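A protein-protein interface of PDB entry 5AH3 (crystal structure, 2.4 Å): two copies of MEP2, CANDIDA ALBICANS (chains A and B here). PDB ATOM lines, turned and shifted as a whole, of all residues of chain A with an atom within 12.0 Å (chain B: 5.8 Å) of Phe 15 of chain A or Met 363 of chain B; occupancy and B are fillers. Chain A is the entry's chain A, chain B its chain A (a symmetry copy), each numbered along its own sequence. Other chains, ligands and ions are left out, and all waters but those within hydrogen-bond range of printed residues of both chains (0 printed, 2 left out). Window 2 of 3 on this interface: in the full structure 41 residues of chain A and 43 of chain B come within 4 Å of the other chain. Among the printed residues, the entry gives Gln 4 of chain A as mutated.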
ATOM      1  N   GLN A   4       4.471  13.002  -7.108  1.00  0.00           N
ATOM      2  CA  GLN A   4       5.912  12.908  -6.913  1.00  0.00           C
ATOM      3  C   GLN A   4       6.398  11.438  -6.963  1.00  0.00           C
ATOM      4  O   GLN A   4       7.588  11.166  -7.119  1.00  0.00           O
ATOM      5  CB  GLN A   4       6.301  13.592  -5.603  1.00  0.00           C
ATOM      6  CG  GLN A   4       7.779  13.617  -5.342  1.00  0.00           C
ATOM      7  CD  GLN A   4       8.453  14.954  -5.523  1.00  0.00           C
ATOM      8  OE1 GLN A   4       9.018  15.236  -6.580  1.00  0.00           O
ATOM      9  NE2 GLN A   4       8.449  15.764  -4.472  1.00  0.00           N
ATOM     10  N   PHE A   5       5.472  10.490  -6.849  1.00  0.00           N
ATOM     11  CA  PHE A   5       5.734   9.121  -7.307  1.00  0.00           C
ATOM     12  C   PHE A   5       5.160   8.993  -8.710  1.00  0.00           C
ATOM     13  O   PHE A   5       3.945   8.991  -8.891  1.00  0.00           O
ATOM     14  CB  PHE A   5       5.103   8.063  -6.396  1.00  0.00           C
ATOM     15  CG  PHE A   5       5.700   7.997  -5.019  1.00  0.00           C
ATOM     16  CD1 PHE A   5       7.026   7.651  -4.837  1.00  0.00           C
ATOM     17  CD2 PHE A   5       4.922   8.256  -3.905  1.00  0.00           C
ATOM     18  CE1 PHE A   5       7.570   7.584  -3.568  1.00  0.00           C
ATOM     19  CE2 PHE A   5       5.462   8.192  -2.634  1.00  0.00           C
ATOM     20  CZ  PHE A   5       6.789   7.852  -2.468  1.00  0.00           C
ATOM     21  N   THR A   6       6.028   8.895  -9.703  1.00  0.00           N
ATOM     22  CA  THR A   6       5.607   8.950 -11.099  1.00  0.00           C
ATOM     23  C   THR A   6       4.891   7.697 -11.613  1.00  0.00           C
ATOM     24  O   THR A   6       4.052   7.782 -12.502  1.00  0.00           O
ATOM     25  CB  THR A   6       6.813   9.206 -12.006  1.00  0.00           C
ATOM     26  OG1 THR A   6       7.679   8.056 -11.984  1.00  0.00           O
ATOM     27  CG2 THR A   6       7.573  10.442 -11.532  1.00  0.00           C
ATOM     28  N   THR A  10      11.928   4.812 -13.541  1.00  0.00           N
ATOM     29  CA  THR A  10      12.475   4.499 -12.225  1.00  0.00           C
ATOM     30  C   THR A  10      11.502   4.680 -11.072  1.00  0.00           C
ATOM     31  O   THR A  10      11.794   4.276  -9.945  1.00  0.00           O
ATOM     32  CB  THR A  10      13.687   5.368 -11.922  1.00  0.00           C
ATOM     33  OG1 THR A  10      13.267   6.735 -11.815  1.00  0.00           O
ATOM     34  CG2 THR A  10      14.720   5.239 -13.028  1.00  0.00           C
ATOM     35  N   GLY A  11      10.364   5.317 -11.340  1.00  0.00           N
ATOM     36  CA  GLY A  11       9.367   5.540 -10.311  1.00  0.00           C
ATOM     37  C   GLY A  11       9.490   6.876  -9.598  1.00  0.00           C
ATOM     38  O   GLY A  11       8.640   7.228  -8.785  1.00  0.00           O
ATOM     39  N   GLY A  12      10.548   7.621  -9.893  1.00  0.00           N
ATOM     40  CA  GLY A  12      10.760   8.906  -9.251  1.00  0.00           C
ATOM     41  C   GLY A  12      12.213   9.165  -8.911  1.00  0.00           C
ATOM     42  O   GLY A  12      13.074   8.324  -9.145  1.00  0.00           O
ATOM     43  N   ASP A  13      12.471  10.333  -8.338  1.00  0.00           N
ATOM     44  CA  ASP A  13      13.815  10.801  -8.026  1.00  0.00           C
ATOM     45  C   ASP A  13      14.205  10.413  -6.599  1.00  0.00           C
ATOM     46  O   ASP A  13      13.658  10.968  -5.640  1.00  0.00           O
ATOM     47  CB  ASP A  13      13.868  12.324  -8.215  1.00  0.00           C
ATOM     48  CG  ASP A  13      15.239  12.922  -7.948  1.00  0.00           C
ATOM     49  OD1 ASP A  13      16.140  12.242  -7.419  1.00  0.00           O
ATOM     50  OD2 ASP A  13      15.411  14.111  -8.265  1.00  0.00           O
ATOM     51  N   VAL A  14      15.160   9.484  -6.467  1.00  0.00           N
ATOM     52  CA  VAL A  14      15.613   8.999  -5.160  1.00  0.00           C
ATOM     53  C   VAL A  14      16.104  10.144  -4.274  1.00  0.00           C
ATOM     54  O   VAL A  14      16.021  10.076  -3.054  1.00  0.00           O
ATOM     55  CB  VAL A  14      16.763   7.914  -5.276  1.00  0.00           C
ATOM     56  CG1 VAL A  14      16.263   6.641  -5.940  1.00  0.00           C
ATOM     57  CG2 VAL A  14      17.997   8.457  -6.003  1.00  0.00           C
ATOM     58  N   PHE A  15      16.614  11.199  -4.889  1.00  0.00           N
ATOM     59  CA  PHE A  15      17.081  12.352  -4.133  1.00  0.00           C
ATOM     60  C   PHE A  15      15.923  13.206  -3.587  1.00  0.00           C
ATOM     61  O   PHE A  15      16.141  14.047  -2.717  1.00  0.00           O
ATOM     62  CB  PHE A  15      18.027  13.198  -4.994  1.00  0.00           C
ATOM     63  CG  PHE A  15      19.340  12.522  -5.285  1.00  0.00           C
ATOM     64  CD1 PHE A  15      20.238  12.259  -4.267  1.00  0.00           C
ATOM     65  CD2 PHE A  15      19.675  12.138  -6.573  1.00  0.00           C
ATOM     66  CE1 PHE A  15      21.447  11.617  -4.525  1.00  0.00           C
ATOM     67  CE2 PHE A  15      20.889  11.493  -6.835  1.00  0.00           C
ATOM     68  CZ  PHE A  15      21.773  11.239  -5.805  1.00  0.00           C
ATOM     69  N   LYS A  16      14.700  12.969  -4.064  1.00  0.00           N
ATOM     70  CA  LYS A  16      13.533  13.708  -3.562  1.00  0.00           C
ATOM     71  C   LYS A  16      12.471  12.843  -2.892  1.00  0.00           C
ATOM     72  O   LYS A  16      11.684  13.345  -2.099  1.00  0.00           O
ATOM     73  CB  LYS A  16      12.867  14.484  -4.686  1.00  0.00           C
ATOM     74  CG  LYS A  16      13.717  15.581  -5.256  1.00  0.00           C
ATOM     75  CD  LYS A  16      12.898  16.445  -6.173  1.00  0.00           C
ATOM     76  CE  LYS A  16      13.709  16.879  -7.365  1.00  0.00           C
ATOM     77  NZ  LYS A  16      13.038  17.980  -8.110  1.00  0.00           N
ATOM     78  N   VAL A  17      12.418  11.559  -3.234  1.00  0.00           N
ATOM     79  CA  VAL A  17      11.471  10.658  -2.587  1.00  0.00           C
ATOM     80  C   VAL A  17      12.067   9.344  -2.171  1.00  0.00           C
ATOM     81  O   VAL A  17      13.014   8.851  -2.779  1.00  0.00           O
ATOM     82  CB  VAL A  17      10.268  10.312  -3.478  1.00  0.00           C
ATOM     83  CG1 VAL A  17       9.452  11.493  -3.683  1.00  0.00           C
ATOM     84  CG2 VAL A  17      10.706   9.718  -4.817  1.00  0.00           C
ATOM     85  N   ASP A  18      11.471   8.781  -1.129  1.00  0.00           N
ATOM     86  CA  ASP A  18      11.699   7.409  -0.762  1.00  0.00           C
ATOM     87  C   ASP A  18      10.761   6.517  -1.573  1.00  0.00           C
ATOM     88  O   ASP A  18       9.573   6.427  -1.273  1.00  0.00           O
ATOM     89  CB  ASP A  18      11.489   7.210   0.738  1.00  0.00           C
ATOM     90  CG  ASP A  18      11.928   5.831   1.204  1.00  0.00           C
ATOM     91  OD1 ASP A  18      12.445   5.058   0.365  1.00  0.00           O
ATOM     92  OD2 ASP A  18      11.764   5.526   2.404  1.00  0.00           O
ATOM     93  N   LEU A  19      11.310   5.861  -2.597  1.00  0.00           N
ATOM     94  CA  LEU A  19      10.543   4.947  -3.447  1.00  0.00           C
ATOM     95  C   LEU A  19      10.000   3.752  -2.659  1.00  0.00           C
ATOM     96  O   LEU A  19       9.017   3.145  -3.056  1.00  0.00           O
ATOM     97  CB  LEU A  19      11.401   4.454  -4.622  1.00  0.00           C
ATOM     98  CG  LEU A  19      11.864   5.532  -5.601  1.00  0.00           C
ATOM     99  CD1 LEU A  19      12.780   4.964  -6.641  1.00  0.00           C
ATOM    100  CD2 LEU A  19      10.680   6.218  -6.264  1.00  0.00           C
ATOM    101  N   ASN A  20      10.637   3.438  -1.535  1.00  0.00           N
ATOM    102  CA  ASN A  20      10.209   2.351  -0.658  1.00  0.00           C
ATOM    103  C   ASN A  20       8.860   2.585   0.058  1.00  0.00           C
ATOM    104  O   ASN A  20       8.208   1.626   0.482  1.00  0.00           O
ATOM    105  CB  ASN A  20      11.302   2.079   0.384  1.00  0.00           C
ATOM    106  CG  ASN A  20      12.631   1.651  -0.246  1.00  0.00           C
ATOM    107  OD1 ASN A  20      12.757   0.538  -0.754  1.00  0.00           O
ATOM    108  ND2 ASN A  20      13.624   2.536  -0.210  1.00  0.00           N
ATOM    109  N   GLU A  21       8.448   3.855   0.187  1.00  0.00           N
ATOM    110  CA  GLU A  21       7.199   4.218   0.857  1.00  0.00           C
ATOM    111  C   GLU A  21       5.979   3.669   0.115  1.00  0.00           C
ATOM    112  O   GLU A  21       4.936   3.447   0.707  1.00  0.00           O
ATOM    113  CB  GLU A  21       7.082   5.742   1.003  1.00  0.00           C
ATOM    114  CG  GLU A  21       7.927   6.366   2.120  1.00  0.00           C
ATOM    115  CD  GLU A  21       7.912   7.900   2.088  1.00  0.00           C
ATOM    116  OE1 GLU A  21       7.065   8.483   1.381  1.00  0.00           O
ATOM    117  OE2 GLU A  21       8.754   8.529   2.767  1.00  0.00           O
ATOM    118  N   GLN A  22       6.133   3.417  -1.177  1.00  0.00           N
ATOM    119  CA  GLN A  22       5.081   2.803  -1.981  1.00  0.00           C
ATOM    120  C   GLN A  22       4.769   1.335  -1.666  1.00  0.00           C
ATOM    121  O   GLN A  22       3.809   0.795  -2.207  1.00  0.00           O
ATOM    122  CB  GLN A  22       5.439   2.885  -3.463  1.00  0.00           C
ATOM    123  CG  GLN A  22       5.751   4.272  -3.984  1.00  0.00           C
ATOM    124  CD  GLN A  22       6.231   4.227  -5.423  1.00  0.00           C
ATOM    125  OE1 GLN A  22       5.453   4.432  -6.353  1.00  0.00           O
ATOM    126  NE2 GLN A  22       7.517   3.937  -5.611  1.00  0.00           N
ATOM    127  N   ARG A  25       6.950  -3.369   3.606  1.00  0.00           N
ATOM    128  CA  ARG A  25       8.286  -3.919   3.711  1.00  0.00           C
ATOM    129  C   ARG A  25       8.271  -5.449   3.832  1.00  0.00           C
ATOM    130  O   ARG A  25       9.125  -6.137   3.274  1.00  0.00           O
ATOM    131  CB  ARG A  25       9.024  -3.311   4.908  1.00  0.00           C
ATOM    132  CG  ARG A  25       9.296  -1.826   4.821  1.00  0.00           C
ATOM    133  CD  ARG A  25      10.005  -1.461   3.543  1.00  0.00           C
ATOM    134  NE  ARG A  25      10.519  -0.097   3.574  1.00  0.00           N
ATOM    135  CZ  ARG A  25      11.750   0.237   3.951  1.00  0.00           C
ATOM    136  NH1 ARG A  25      12.606  -0.694   4.338  1.00  0.00           N
ATOM    137  NH2 ARG A  25      12.127   1.506   3.937  1.00  0.00           N
ATOM    138  N   LEU A 105      13.758  -0.005 -11.546  1.00  0.00           N
ATOM    139  CA  LEU A 105      14.020   0.353 -10.163  1.00  0.00           C
ATOM    140  C   LEU A 105      12.748   0.320  -9.332  1.00  0.00           C
ATOM    141  O   LEU A 105      12.278  -0.758  -8.959  1.00  0.00           O
ATOM    142  CB  LEU A 105      14.692   1.732 -10.081  1.00  0.00           C
ATOM    143  CG  LEU A 105      15.195   2.218  -8.708  1.00  0.00           C
ATOM    144  CD1 LEU A 105      16.092   1.196  -8.040  1.00  0.00           C
ATOM    145  CD2 LEU A 105      15.908   3.554  -8.813  1.00  0.00           C
ATOM    146  N   GLY A 106      12.183   1.497  -9.061  1.00  0.00           N
ATOM    147  CA  GLY A 106      11.217   1.642  -7.991  1.00  0.00           C
ATOM    148  C   GLY A 106       9.766   1.879  -8.351  1.00  0.00           C
ATOM    149  O   GLY A 106       8.940   2.069  -7.468  1.00  0.00           O
ATOM    150  N   ILE A 117      12.546  -3.773  -9.634  1.00  0.00           N
ATOM    151  CA  ILE A 117      13.822  -4.428  -9.405  1.00  0.00           C
ATOM    152  C   ILE A 117      13.673  -5.737  -8.599  1.00  0.00           C
ATOM    153  O   ILE A 117      14.438  -6.672  -8.802  1.00  0.00           O
ATOM    154  CB  ILE A 117      14.830  -3.456  -8.700  1.00  0.00           C
ATOM    155  CG1 ILE A 117      16.259  -4.020  -8.735  1.00  0.00           C
ATOM    156  CG2 ILE A 117      14.379  -3.101  -7.283  1.00  0.00           C
ATOM    157  CD1 ILE A 117      16.878  -4.110 -10.132  1.00  0.00           C
ATOM    158  N   ARG B 250      17.114  -1.546  -2.075  1.00  0.00           N
ATOM    159  CA  ARG B 250      18.547  -1.566  -2.329  1.00  0.00           C
ATOM    160  C   ARG B 250      19.077  -2.990  -2.075  1.00  0.00           C
ATOM    161  O   ARG B 250      20.022  -3.435  -2.724  1.00  0.00           O
ATOM    162  CB  ARG B 250      19.311  -0.538  -1.473  1.00  0.00           C
ATOM    163  CG  ARG B 250      20.787  -0.395  -1.926  1.00  0.00           C
ATOM    164  CD  ARG B 250      21.558   0.821  -1.383  1.00  0.00           C
ATOM    165  NE  ARG B 250      21.984   0.650   0.002  1.00  0.00           N
ATOM    166  CZ  ARG B 250      23.245   0.643   0.422  1.00  0.00           C
ATOM    167  NH1 ARG B 250      24.241   0.796  -0.436  1.00  0.00           N
ATOM    168  NH2 ARG B 250      23.507   0.486   1.712  1.00  0.00           N
ATOM    169  N   ALA B 358      28.131   4.844  -7.347  1.00  0.00           N
ATOM    170  CA  ALA B 358      27.250   5.939  -7.745  1.00  0.00           C
ATOM    171  C   ALA B 358      26.348   6.384  -6.592  1.00  0.00           C
ATOM    172  O   ALA B 358      25.636   5.560  -6.011  1.00  0.00           O
ATOM    173  CB  ALA B 358      26.414   5.522  -8.937  1.00  0.00           C
ATOM    174  N   ASP B 359      26.361   7.683  -6.275  1.00  0.00           N
ATOM    175  CA  ASP B 359      25.624   8.189  -5.109  1.00  0.00           C
ATOM    176  C   ASP B 359      24.124   7.943  -5.221  1.00  0.00           C
ATOM    177  O   ASP B 359      23.462   7.739  -4.212  1.00  0.00           O
ATOM    178  CB  ASP B 359      25.898   9.694  -4.855  1.00  0.00           C
ATOM    179  CG  ASP B 359      25.521  10.592  -6.032  1.00  0.00           C
ATOM    180  OD1 ASP B 359      24.839  10.148  -6.968  1.00  0.00           O
ATOM    181  OD2 ASP B 359      25.922  11.769  -6.024  1.00  0.00           O
ATOM    182  N   TYR B 360      23.591   7.935  -6.435  1.00  0.00           N
ATOM    183  CA  TYR B 360      22.169   7.660  -6.612  1.00  0.00           C
ATOM    184  C   TYR B 360      21.792   6.180  -6.473  1.00  0.00           C
ATOM    185  O   TYR B 360      20.615   5.876  -6.294  1.00  0.00           O
ATOM    186  CB  TYR B 360      21.688   8.183  -7.964  1.00  0.00           C
ATOM    187  CG  TYR B 360      22.465   7.681  -9.156  1.00  0.00           C
ATOM    188  CD1 TYR B 360      22.237   6.409  -9.667  1.00  0.00           C
ATOM    189  CD2 TYR B 360      23.408   8.490  -9.792  1.00  0.00           C
ATOM    190  CE1 TYR B 360      22.928   5.944 -10.760  1.00  0.00           C
ATOM    191  CE2 TYR B 360      24.114   8.031 -10.894  1.00  0.00           C
ATOM    192  CZ  TYR B 360      23.868   6.753 -11.369  1.00  0.00           C
ATOM    193  OH  TYR B 360      24.544   6.272 -12.459  1.00  0.00           O
ATOM    194  N   VAL B 361      22.768   5.265  -6.577  1.00  0.00           N
ATOM    195  CA  VAL B 361      22.530   3.858  -6.257  1.00  0.00           C
ATOM    196  C   VAL B 361      22.459   3.707  -4.742  1.00  0.00           C
ATOM    197  O   VAL B 361      21.547   3.089  -4.207  1.00  0.00           O
ATOM    198  CB  VAL B 361      23.637   2.901  -6.806  1.00  0.00           C
ATOM    199  CG1 VAL B 361      23.458   1.510  -6.231  1.00  0.00           C
ATOM    200  CG2 VAL B 361      23.635   2.845  -8.314  1.00  0.00           C
ATOM    201  N   ALA B 362      23.440   4.274  -4.051  1.00  0.00           N
ATOM    202  CA  ALA B 362      23.396   4.330  -2.597  1.00  0.00           C
ATOM    203  C   ALA B 362      22.112   5.009  -2.089  1.00  0.00           C
ATOM    204  O   ALA B 362      21.504   4.533  -1.131  1.00  0.00           O
ATOM    205  CB  ALA B 362      24.628   5.055  -2.060  1.00  0.00           C
ATOM    206  N   MET B 363      21.691   6.096  -2.742  1.00  0.00           N
ATOM    207  CA  MET B 363      20.549   6.890  -2.267  1.00  0.00           C
ATOM    208  C   MET B 363      19.206   6.123  -2.321  1.00  0.00           C
ATOM    209  O   MET B 363      18.228   6.547  -1.713  1.00  0.00           O
ATOM    210  CB  MET B 363      20.464   8.205  -3.066  1.00  0.00           C
ATOM    211  CG  MET B 363      19.419   9.237  -2.604  1.00  0.00           C
ATOM    212  SD  MET B 363      19.399   9.689  -0.847  1.00  0.00           S
ATOM    213  CE  MET B 363      21.040  10.324  -0.572  1.00  0.00           C
ATOM    214  N   ILE B 364      19.172   4.984  -3.017  1.00  0.00           N
ATOM    215  CA  ILE B 364      17.962   4.161  -3.127  1.00  0.00           C
ATOM    216  C   ILE B 364      17.273   3.899  -1.774  1.00  0.00           C
ATOM    217  O   ILE B 364      16.048   3.797  -1.696  1.00  0.00           O
ATOM    218  CB  ILE B 364      18.288   2.790  -3.805  1.00  0.00           C
ATOM    219  CG1 ILE B 364      18.616   2.983  -5.287  1.00  0.00           C
ATOM    220  CG2 ILE B 364      17.147   1.800  -3.644  1.00  0.00           C
ATOM    221  CD1 ILE B 364      19.161   1.713  -5.971  1.00  0.00           C
ATOM    222  N   ASP B 365      18.065   3.793  -0.713  1.00  0.00           N
ATOM    223  CA  ASP B 365      17.531   3.647   0.635  1.00  0.00           C
ATOM    224  C   ASP B 365      17.995   4.778   1.569  1.00  0.00           C
ATOM    225  O   ASP B 365      17.961   4.640   2.786  1.00  0.00           O
ATOM    226  CB  ASP B 365      17.929   2.287   1.216  1.00  0.00           C
ATOM    227  CG  ASP B 365      19.424   2.153   1.443  1.00  0.00           C
ATOM    228  OD1 ASP B 365      20.192   3.049   1.038  1.00  0.00           O
ATOM    229  OD2 ASP B 365      19.839   1.129   2.025  1.00  0.00           O
ATOM    230  N   GLY B 366      18.456   5.882   0.995  1.00  0.00           N
ATOM    231  CA  GLY B 366      18.824   7.043   1.790  1.00  0.00           C
ATOM    232  C   GLY B 366      20.281   7.133   2.221  1.00  0.00           C
ATOM    233  O   GLY B 366      20.671   8.078   2.903  1.00  0.00           O
ATOM    234  N   THR B 367      21.083   6.151   1.821  1.00  0.00           N
ATOM    235  CA  THR B 367      22.505   6.114   2.143  1.00  0.00           C
ATOM    236  C   THR B 367      23.227   7.185   1.352  1.00  0.00           C
ATOM    237  O   THR B 367      22.994   7.345   0.149  1.00  0.00           O
ATOM    238  CB  THR B 367      23.128   4.719   1.832  1.00  0.00           C
ATOM    239  OG1 THR B 367      22.378   3.706   2.504  1.00  0.00           O
ATOM    240  CG2 THR B 367      24.579   4.650   2.290  1.00  0.00           C
ATOM    241  N   GLU B 368      24.106   7.918   2.026  1.00  0.00           N
ATOM    242  CA  GLU B 368      24.769   9.053   1.398  1.00  0.00           C
ATOM    243  C   GLU B 368      26.252   8.815   1.212  1.00  0.00           C
ATOM    244  O   GLU B 368      26.981   8.596   2.174  1.00  0.00           O
ATOM    245  CB  GLU B 368      24.547  10.330   2.224  1.00  0.00           C
ATOM    246  CG  GLU B 368      23.074  10.628   2.483  1.00  0.00           C
ATOM    247  CD  GLU B 368      22.856  11.906   3.286  1.00  0.00           C
ATOM    248  OE1 GLU B 368      23.776  12.336   4.009  1.00  0.00           O
ATOM    249  OE2 GLU B 368      21.751  12.481   3.194  1.00  0.00           O
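ND2 of Asn 20 of chain A is in hydrogen-bond range of O of Ile 364 of chain B (3.1 Å).
N of Ile 117 of chain A lies within hydrogen-bond range of O of Leu 105 of chain A.
The side-chain carboxylate of Asp 18 of chain A lies within hydrogen-bond range of the side-chain amide nitrogen of Asn 20 of chain A.
The backbone NH (N) of Phe 15 of chain A is in hydrogen-bond range of the side-chain carboxylate (OD1) of Asp 13 of chain A (2.8 Å).
Val 14 of chain A touches Tyr 360 of chain B.
Val 14 of chain A touches Met 363 of chain B (O to CG, 3.5 Å).
Phe 15 of chain A touches Asp 359 of chain B (CZ to OD1, 3.5 Å).
Tyr 360 of chain B touches Phe 15 of chain A.
Met 363 of chain B touches Phe 15 of chain A.
Ile 364 of chain B touches Leu 105 of chain A (CD1 to CD1, 3.7 Å).
Of chain B, only Asp 359 (3.5 Å), Tyr 360 (3.6 Å) and Met 363 (3.5 Å) come within 4 Å of Phe 15 of chain A.
Printed residues of chain B within 4 Å of Asn 20 of chain A: Ile 364.
Glu 21 of chain A touches none of the printed residues of chain B.
Of the printed residues of chain B, Leu 105 of chain A touches Ile 364 (3.7 Å).
Of the printed residues of chain A, Tyr 360 of chain B touches Val 14 and Phe 15.
No residue of chain A comes within 4 Å of Val 361 of chain B.
No residue of chain A comes within 4 Å of Ala 362 of chain B.
Met 363 of chain B touches two residues of chain A.
Ile 364 of chain B touches just these residues of chain A: Asn 20 and Leu 105.
No residue of chain A comes within 4 Å of Asp 365 of chain B.
No residue of chain A comes within 4 Å of Gly 366 of chain B.
The nearest printed residue of chain B that does not touch Phe 15 of chain A is Val 361 of chain B (6.1 Å).
The nearest residue of chain A that does not touch Met 363 of chain B is Val 17 of chain A (5.8 Å).
Printed residues of chain B that touch a printed residue of chain A: Asp 359, Tyr 360, Met 363 and Ile 364.
Hydrophobic or aromatic side chains of chain B within 4 Å of the printed part of chain A: Tyr 360, Met 363 and Ile 364.
Hydrophobic or aromatic side chains of chain A that line the printed part of chain B: Val 14, Phe 15 and Leu 105.
No position is printed for both chains.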
